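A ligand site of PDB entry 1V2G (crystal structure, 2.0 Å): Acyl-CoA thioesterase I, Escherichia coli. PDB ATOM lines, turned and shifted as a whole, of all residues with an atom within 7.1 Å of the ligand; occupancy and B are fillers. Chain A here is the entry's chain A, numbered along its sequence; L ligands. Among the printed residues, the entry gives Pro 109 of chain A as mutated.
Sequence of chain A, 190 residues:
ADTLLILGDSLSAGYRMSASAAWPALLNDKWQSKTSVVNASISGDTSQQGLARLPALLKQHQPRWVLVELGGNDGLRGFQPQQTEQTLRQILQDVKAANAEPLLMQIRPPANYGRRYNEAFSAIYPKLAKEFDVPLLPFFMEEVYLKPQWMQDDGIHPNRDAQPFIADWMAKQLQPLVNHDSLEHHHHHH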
ATOM      1  N   GLY A   8      10.857 -30.412  14.160  1.00  0.00           N
ATOM      2  CA  GLY A   8       9.963 -30.228  13.041  1.00  0.00           C
ATOM      3  C   GLY A   8      10.104 -31.221  11.901  1.00  0.00           C
ATOM      4  O   GLY A   8      10.768 -32.254  12.035  1.00  0.00           O
ATOM      5  N   ASP A   9       9.462 -30.884  10.780  1.00  0.00           N
ATOM      6  CA  ASP A   9       9.499 -31.732   9.605  1.00  0.00           C
ATOM      7  C   ASP A   9      10.320 -31.072   8.509  1.00  0.00           C
ATOM      8  O   ASP A   9      11.266 -30.336   8.786  1.00  0.00           O
ATOM      9  CB  ASP A   9       8.072 -32.063   9.114  1.00  0.00           C
ATOM     10  CG  ASP A   9       7.158 -30.841   9.045  1.00  0.00           C
ATOM     11  OD1 ASP A   9       7.615 -29.776   8.571  1.00  0.00           O
ATOM     12  OD2 ASP A   9       5.981 -30.935   9.450  1.00  0.00           O
ATOM     13  N   SER A  10       9.950 -31.348   7.261  1.00  0.00           N
ATOM     14  CA  SER A  10      10.677 -30.807   6.112  1.00  0.00           C
ATOM     15  C   SER A  10      10.712 -29.277   6.098  1.00  0.00           C
ATOM     16  O   SER A  10      11.667 -28.668   5.611  1.00  0.00           O
ATOM     17  CB  SER A  10      10.049 -31.325   4.814  1.00  0.00           C
ATOM     18  OG  SER A  10      10.793 -30.969   3.682  1.00  0.00           O
ATOM     19  N   LEU A  11       9.665 -28.640   6.634  1.00  0.00           N
ATOM     20  CA  LEU A  11       9.653 -27.184   6.637  1.00  0.00           C
ATOM     21  C   LEU A  11      10.866 -26.653   7.392  1.00  0.00           C
ATOM     22  O   LEU A  11      11.375 -25.581   7.076  1.00  0.00           O
ATOM     23  CB  LEU A  11       8.349 -26.664   7.246  1.00  0.00           C
ATOM     24  CG  LEU A  11       7.119 -26.980   6.388  1.00  0.00           C
ATOM     25  CD1 LEU A  11       5.908 -26.297   7.001  1.00  0.00           C
ATOM     26  CD2 LEU A  11       7.321 -26.514   4.940  1.00  0.00           C
ATOM     27  N   SER A  12      11.335 -27.412   8.371  1.00  0.00           N
ATOM     28  CA  SER A  12      12.505 -27.005   9.140  1.00  0.00           C
ATOM     29  C   SER A  12      13.768 -27.766   8.729  1.00  0.00           C
ATOM     30  O   SER A  12      14.868 -27.233   8.839  1.00  0.00           O
ATOM     31  CB  SER A  12      12.241 -27.168  10.633  1.00  0.00           C
ATOM     32  OG  SER A  12      11.212 -26.301  11.050  1.00  0.00           O
ATOM     33  N   ALA A  13      13.611 -29.000   8.255  1.00  0.00           N
ATOM     34  CA  ALA A  13      14.764 -29.795   7.844  1.00  0.00           C
ATOM     35  C   ALA A  13      15.246 -29.374   6.481  1.00  0.00           C
ATOM     36  O   ALA A  13      16.423 -29.512   6.163  1.00  0.00           O
ATOM     37  CB  ALA A  13      14.415 -31.278   7.836  1.00  0.00           C
ATOM     38  N   TYR A  15      13.577 -29.228   2.274  1.00  0.00           N
ATOM     39  CA  TYR A  15      13.082 -30.244   1.349  1.00  0.00           C
ATOM     40  C   TYR A  15      13.941 -30.310   0.101  1.00  0.00           C
ATOM     41  O   TYR A  15      14.087 -29.344  -0.617  1.00  0.00           O
ATOM     42  CB  TYR A  15      11.640 -29.928   0.954  1.00  0.00           C
ATOM     43  CG  TYR A  15      10.992 -30.985   0.085  1.00  0.00           C
ATOM     44  CD1 TYR A  15      10.841 -30.779  -1.300  1.00  0.00           C
ATOM     45  CD2 TYR A  15      10.516 -32.175   0.628  1.00  0.00           C
ATOM     46  CE1 TYR A  15      10.231 -31.734  -2.100  1.00  0.00           C
ATOM     47  CE2 TYR A  15       9.903 -33.147  -0.176  1.00  0.00           C
ATOM     48  CZ  TYR A  15       9.763 -32.912  -1.541  1.00  0.00           C
ATOM     49  OH  TYR A  15       9.162 -33.862  -2.343  1.00  0.00           O
ATOM     50  N   ILE A  42      13.037 -33.827  10.575  1.00  0.00           N
ATOM     51  CA  ILE A  42      13.182 -34.851   9.543  1.00  0.00           C
ATOM     52  C   ILE A  42      12.017 -34.753   8.571  1.00  0.00           C
ATOM     53  O   ILE A  42      10.867 -34.746   8.993  1.00  0.00           O
ATOM     54  CB  ILE A  42      13.223 -36.271  10.169  1.00  0.00           C
ATOM     55  CG1 ILE A  42      14.379 -36.363  11.171  1.00  0.00           C
ATOM     56  CG2 ILE A  42      13.391 -37.321   9.062  1.00  0.00           C
ATOM     57  CD1 ILE A  42      14.433 -37.699  11.926  1.00  0.00           C
ATOM     58  N   SER A  43      12.332 -34.667   7.280  1.00  0.00           N
ATOM     59  CA  SER A  43      11.274 -34.565   6.265  1.00  0.00           C
ATOM     60  C   SER A  43      10.301 -35.720   6.381  1.00  0.00           C
ATOM     61  O   SER A  43      10.699 -36.858   6.637  1.00  0.00           O
ATOM     62  CB  SER A  43      11.881 -34.558   4.857  1.00  0.00           C
ATOM     63  OG  SER A  43      12.676 -33.393   4.649  1.00  0.00           O
ATOM     64  N   GLY A  44       9.009 -35.421   6.209  1.00  0.00           N
ATOM     65  CA  GLY A  44       7.977 -36.434   6.271  1.00  0.00           C
ATOM     66  C   GLY A  44       7.520 -36.826   7.665  1.00  0.00           C
ATOM     67  O   GLY A  44       6.547 -37.564   7.816  1.00  0.00           O
ATOM     68  N   ASP A  45       8.204 -36.341   8.688  1.00  0.00           N
ATOM     69  CA  ASP A  45       7.841 -36.678  10.063  1.00  0.00           C
ATOM     70  C   ASP A  45       6.456 -36.164  10.439  1.00  0.00           C
ATOM     71  O   ASP A  45       6.084 -35.033  10.122  1.00  0.00           O
ATOM     72  CB  ASP A  45       8.860 -36.133  11.057  1.00  0.00           C
ATOM     73  CG  ASP A  45       9.671 -37.226  11.729  1.00  0.00           C
ATOM     74  OD1 ASP A  45       9.992 -38.225  11.043  1.00  0.00           O
ATOM     75  OD2 ASP A  45      10.011 -37.080  12.919  1.00  0.00           O
ATOM     76  N   THR A  46       5.711 -37.023  11.120  1.00  0.00           N
ATOM     77  CA  THR A  46       4.377 -36.696  11.610  1.00  0.00           C
ATOM     78  C   THR A  46       4.577 -36.278  13.059  1.00  0.00           C
ATOM     79  O   THR A  46       5.661 -36.466  13.615  1.00  0.00           O
ATOM     80  CB  THR A  46       3.452 -37.918  11.603  1.00  0.00           C
ATOM     81  OG1 THR A  46       3.973 -38.914  12.502  1.00  0.00           O
ATOM     82  CG2 THR A  46       3.335 -38.500  10.207  1.00  0.00           C
ATOM     83  N   GLU A  69       7.259 -27.679  15.419  1.00  0.00           N
ATOM     84  CA  GLU A  69       6.723 -27.419  14.082  1.00  0.00           C
ATOM     85  C   GLU A  69       6.353 -28.762  13.465  1.00  0.00           C
ATOM     86  O   GLU A  69       7.109 -29.318  12.659  1.00  0.00           O
ATOM     87  CB  GLU A  69       7.768 -26.695  13.221  1.00  0.00           C
ATOM     88  CG  GLU A  69       7.273 -26.304  11.825  1.00  0.00           C
ATOM     89  CD  GLU A  69       7.604 -27.352  10.773  1.00  0.00           C
ATOM     90  OE1 GLU A  69       6.689 -27.752  10.004  1.00  0.00           O
ATOM     91  OE2 GLU A  69       8.776 -27.775  10.702  1.00  0.00           O
ATOM     92  N   GLY A  71       2.723 -31.567  12.474  1.00  0.00           N
ATOM     93  CA  GLY A  71       1.295 -31.720  12.247  1.00  0.00           C
ATOM     94  C   GLY A  71       0.954 -31.660  10.776  1.00  0.00           C
ATOM     95  O   GLY A  71      -0.008 -32.265  10.341  1.00  0.00           O
ATOM     96  N   GLY A  72       1.755 -30.906  10.018  1.00  0.00           N
ATOM     97  CA  GLY A  72       1.515 -30.762   8.590  1.00  0.00           C
ATOM     98  C   GLY A  72       1.461 -32.064   7.801  1.00  0.00           C
ATOM     99  O   GLY A  72       0.849 -32.104   6.728  1.00  0.00           O
ATOM    100  N   ASN A  73       2.094 -33.113   8.304  1.00  0.00           N
ATOM    101  CA  ASN A  73       2.102 -34.419   7.624  1.00  0.00           C
ATOM    102  C   ASN A  73       0.957 -35.328   8.115  1.00  0.00           C
ATOM    103  O   ASN A  73       0.557 -36.249   7.401  1.00  0.00           O
ATOM    104  CB  ASN A  73       3.447 -35.156   7.846  1.00  0.00           C
ATOM    105  CG  ASN A  73       4.600 -34.585   7.023  1.00  0.00           C
ATOM    106  OD1 ASN A  73       5.655 -34.241   7.569  1.00  0.00           O
ATOM    107  ND2 ASN A  73       4.425 -34.495   5.702  1.00  0.00           N
ATOM    108  N   ILE A 107       0.056 -24.397  12.368  1.00  0.00           N
ATOM    109  CA  ILE A 107       0.199 -25.099  11.096  1.00  0.00           C
ATOM    110  C   ILE A 107      -1.153 -25.012  10.382  1.00  0.00           C
ATOM    111  O   ILE A 107      -2.213 -25.060  11.029  1.00  0.00           O
ATOM    112  CB  ILE A 107       0.595 -26.575  11.298  1.00  0.00           C
ATOM    113  CG1 ILE A 107       1.931 -26.678  12.061  1.00  0.00           C
ATOM    114  CG2 ILE A 107       0.752 -27.250   9.941  1.00  0.00           C
ATOM    115  CD1 ILE A 107       3.132 -26.182  11.256  1.00  0.00           C
ATOM    116  N   ARG A 108      -1.130 -24.880   9.059  1.00  0.00           N
ATOM    117  CA  ARG A 108      -2.361 -24.806   8.267  1.00  0.00           C
ATOM    118  C   ARG A 108      -2.245 -25.737   7.071  1.00  0.00           C
ATOM    119  O   ARG A 108      -1.321 -25.610   6.274  1.00  0.00           O
ATOM    120  CB  ARG A 108      -2.632 -23.382   7.786  1.00  0.00           C
ATOM    121  CG  ARG A 108      -3.908 -23.268   6.946  1.00  0.00           C
ATOM    122  CD  ARG A 108      -4.260 -21.814   6.613  1.00  0.00           C
ATOM    123  NE  ARG A 108      -3.385 -21.240   5.592  1.00  0.00           N
ATOM    124  CZ  ARG A 108      -3.454 -21.524   4.298  1.00  0.00           C
ATOM    125  NH1 ARG A 108      -4.358 -22.377   3.841  1.00  0.00           N
ATOM    126  NH2 ARG A 108      -2.622 -20.934   3.453  1.00  0.00           N
ATOM    127  N   PRO A 109      -3.184 -26.684   6.916  1.00  0.00           N
ATOM    128  CA  PRO A 109      -3.173 -27.628   5.799  1.00  0.00           C
ATOM    129  C   PRO A 109      -3.529 -26.974   4.454  1.00  0.00           C
ATOM    130  O   PRO A 109      -4.011 -25.853   4.429  1.00  0.00           O
ATOM    131  CB  PRO A 109      -4.184 -28.686   6.231  1.00  0.00           C
ATOM    132  CG  PRO A 109      -5.184 -27.869   6.988  1.00  0.00           C
ATOM    133  CD  PRO A 109      -4.328 -26.943   7.813  1.00  0.00           C
ATOM    134  N   PRO A 110      -3.298 -27.673   3.332  1.00  0.00           N
ATOM    135  CA  PRO A 110      -3.609 -27.103   2.020  1.00  0.00           C
ATOM    136  C   PRO A 110      -5.066 -26.658   1.918  1.00  0.00           C
ATOM    137  O   PRO A 110      -5.962 -27.302   2.473  1.00  0.00           O
ATOM    138  CB  PRO A 110      -3.289 -28.256   1.072  1.00  0.00           C
ATOM    139  CG  PRO A 110      -2.159 -28.944   1.754  1.00  0.00           C
ATOM    140  CD  PRO A 110      -2.645 -28.987   3.187  1.00  0.00           C
ATOM    141  N   ALA A 111      -5.291 -25.550   1.226  1.00  0.00           N
ATOM    142  CA  ALA A 111      -6.640 -25.006   1.067  1.00  0.00           C
ATOM    143  C   ALA A 111      -7.618 -26.059   0.545  1.00  0.00           C
ATOM    144  O   ALA A 111      -8.821 -25.955   0.758  1.00  0.00           O
ATOM    145  CB  ALA A 111      -6.610 -23.807   0.108  1.00  0.00           C
ATOM    146  N   TYR A 113      -8.211 -29.447   1.377  1.00  0.00           N
ATOM    147  CA  TYR A 113      -8.161 -30.617   2.240  1.00  0.00           C
ATOM    148  C   TYR A 113      -9.484 -30.760   2.994  1.00  0.00           C
ATOM    149  O   TYR A 113      -9.584 -31.542   3.943  1.00  0.00           O
ATOM    150  CB  TYR A 113      -7.008 -30.525   3.236  1.00  0.00           C
ATOM    151  CG  TYR A 113      -5.861 -31.507   3.003  1.00  0.00           C
ATOM    152  CD1 TYR A 113      -4.834 -31.623   3.937  1.00  0.00           C
ATOM    153  CD2 TYR A 113      -5.815 -32.299   1.860  1.00  0.00           C
ATOM    154  CE1 TYR A 113      -3.772 -32.512   3.732  1.00  0.00           C
ATOM    155  CE2 TYR A 113      -4.770 -33.201   1.649  1.00  0.00           C
ATOM    156  CZ  TYR A 113      -3.745 -33.293   2.585  1.00  0.00           C
ATOM    157  OH  TYR A 113      -2.710 -34.175   2.378  1.00  0.00           O
ATOM    158  N   PHE A 139       2.241 -19.213  11.269  1.00  0.00           N
ATOM    159  CA  PHE A 139       2.757 -20.196  10.323  1.00  0.00           C
ATOM    160  C   PHE A 139       3.604 -19.400   9.336  1.00  0.00           C
ATOM    161  O   PHE A 139       3.058 -18.657   8.511  1.00  0.00           O
ATOM    162  CB  PHE A 139       1.596 -20.898   9.623  1.00  0.00           C
ATOM    163  CG  PHE A 139       2.014 -22.023   8.708  1.00  0.00           C
ATOM    164  CD1 PHE A 139       3.082 -22.859   9.018  1.00  0.00           C
ATOM    165  CD2 PHE A 139       1.247 -22.304   7.575  1.00  0.00           C
ATOM    166  CE1 PHE A 139       3.387 -23.956   8.208  1.00  0.00           C
ATOM    167  CE2 PHE A 139       1.543 -23.405   6.767  1.00  0.00           C
ATOM    168  CZ  PHE A 139       2.620 -24.233   7.084  1.00  0.00           C
ATOM    169  N   MET A 141       5.002 -20.157   6.656  1.00  0.00           N
ATOM    170  CA  MET A 141       4.703 -20.410   5.251  1.00  0.00           C
ATOM    171  C   MET A 141       3.650 -19.458   4.661  1.00  0.00           C
ATOM    172  O   MET A 141       3.588 -19.307   3.437  1.00  0.00           O
ATOM    173  CB  MET A 141       4.290 -21.875   5.043  1.00  0.00           C
ATOM    174  CG  MET A 141       5.440 -22.886   5.088  1.00  0.00           C
ATOM    175  SD  MET A 141       6.783 -22.462   3.917  1.00  0.00           S
ATOM    176  CE  MET A 141       5.943 -22.681   2.321  1.00  0.00           C
ATOM    177  N   TYR A 145       4.040 -18.262   0.745  1.00  0.00           N
ATOM    178  CA  TYR A 145       3.073 -18.498  -0.322  1.00  0.00           C
ATOM    179  C   TYR A 145       2.864 -17.245  -1.155  1.00  0.00           C
ATOM    180  O   TYR A 145       2.567 -17.325  -2.348  1.00  0.00           O
ATOM    181  CB  TYR A 145       1.711 -18.901   0.252  1.00  0.00           C
ATOM    182  CG  TYR A 145       1.707 -20.204   0.994  1.00  0.00           C
ATOM    183  CD1 TYR A 145       0.875 -20.374   2.107  1.00  0.00           C
ATOM    184  CD2 TYR A 145       2.486 -21.286   0.581  1.00  0.00           C
ATOM    185  CE1 TYR A 145       0.817 -21.592   2.773  1.00  0.00           C
ATOM    186  CE2 TYR A 145       2.437 -22.499   1.244  1.00  0.00           C
ATOM    187  CZ  TYR A 145       1.597 -22.640   2.347  1.00  0.00           C
ATOM    188  OH  TYR A 145       1.543 -23.841   3.017  1.00  0.00           O
ATOM    189  N   GLY A 155       4.539 -26.667  -4.987  1.00  0.00           N
ATOM    190  CA  GLY A 155       3.712 -25.647  -4.358  1.00  0.00           C
ATOM    191  C   GLY A 155       3.415 -25.905  -2.894  1.00  0.00           C
ATOM    192  O   GLY A 155       2.429 -25.387  -2.344  1.00  0.00           O
ATOM    193  N   ILE A 156       4.283 -26.683  -2.256  1.00  0.00           N
ATOM    194  CA  ILE A 156       4.147 -27.035  -0.850  1.00  0.00           C
ATOM    195  C   ILE A 156       5.387 -26.646  -0.020  1.00  0.00           C
ATOM    196  O   ILE A 156       5.266 -26.091   1.062  1.00  0.00           O
ATOM    197  CB  ILE A 156       3.939 -28.557  -0.681  1.00  0.00           C
ATOM    198  CG1 ILE A 156       2.621 -28.988  -1.325  1.00  0.00           C
ATOM    199  CG2 ILE A 156       3.928 -28.939   0.791  1.00  0.00           C
ATOM    200  CD1 ILE A 156       2.444 -30.495  -1.364  1.00  0.00           C
ATOM    201  N   HIS A 157       6.584 -26.947  -0.532  1.00  0.00           N
ATOM    202  CA  HIS A 157       7.791 -26.658   0.197  1.00  0.00           C
ATOM    203  C   HIS A 157       8.546 -25.416  -0.266  1.00  0.00           C
ATOM    204  O   HIS A 157       8.580 -25.114  -1.461  1.00  0.00           O
ATOM    205  CB  HIS A 157       8.746 -27.873   0.147  1.00  0.00           C
ATOM    206  CG  HIS A 157       8.120 -29.157   0.606  1.00  0.00           C
ATOM    207  ND1 HIS A 157       7.571 -30.065  -0.276  1.00  0.00           N
ATOM    208  CD2 HIS A 157       7.954 -29.682   1.841  1.00  0.00           C
ATOM    209  CE1 HIS A 157       7.102 -31.097   0.400  1.00  0.00           C
ATOM    210  NE2 HIS A 157       7.322 -30.894   1.684  1.00  0.00           N
HETATM  211  C1  LIG L   1       6.892 -32.280   5.277  1.00  0.00           C
HETATM  212  C2  LIG L   1       5.576 -31.550   5.571  1.00  0.00           C
HETATM  213  C3  LIG L   1       5.307 -30.194   4.912  1.00  0.00           C
HETATM  214  C4  LIG L   1       4.087 -29.589   5.598  1.00  0.00           C
HETATM  215  C5  LIG L   1       3.022 -29.216   4.576  1.00  0.00           C
HETATM  216  C6  LIG L   1       1.747 -28.581   5.142  1.00  0.00           C
HETATM  217  C7  LIG L   1       1.497 -27.217   4.535  1.00  0.00           C
HETATM  218  C8  LIG L   1       0.618 -27.134   3.262  1.00  0.00           C
HETATM  219  O1  LIG L   1       7.357 -32.478   4.138  1.00  0.00           O
HETATM  220  O2  LIG L   1       7.878 -32.931   5.879  1.00  0.00           O
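O2 of the ligand sits at hydrogen-bond distance from N of Gly 44, 2.8 Å away. O2 of the ligand sits close to N of Ser 10, at 3.0 Å. An oxygen (O1) of the ligand is in hydrogen-bond range of a ring nitrogen (NE2) of His 157, at 2.9 Å. The side-chain amide oxygen of Asn 73 lies close to an oxygen (O2) of the ligand (3.1 Å).
The backbone carbonyl oxygen of Gly 44 lies close to the side-chain amide oxygen of Asn 73 (3.4 Å). OG of Ser 10 sits at hydrogen-bond distance from OG of Ser 43 (3.2 Å). The side-chain amide oxygen of Asn 73 lies close to the backbone carbonyl oxygen of Asp 45 (2.7 Å). OD1 of Asp 9 is in hydrogen-bond range of N of Leu 11, 3.0 Å away. The side-chain carboxylate of Glu 69 lies within hydrogen-bond range of the backbone NH of Asp 9 (3.2 Å).
Asp 9 touches the ligand. Leu 11 touches the ligand (CG to C3, 3.97 Å). Ser 43 touches the ligand (C to O2, 3.7 Å). Gly 72 touches the ligand. Arg 108 touches the ligand. Pro 110 touches the ligand (CG to C8, 3.6 Å). Tyr 145 touches the ligand (OH to C8, 3.4 Å). Ile 156 touches the ligand. Hydrophobic or aromatic side chains within 4 Å of the ligand: Leu 11, Pro 110, Ile 156 and His 157. Of the 28 residues printed, 12 come within 4 Å of the ligand. The nearest printed residue that does not touch the ligand is Phe 139 (4.1 Å).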
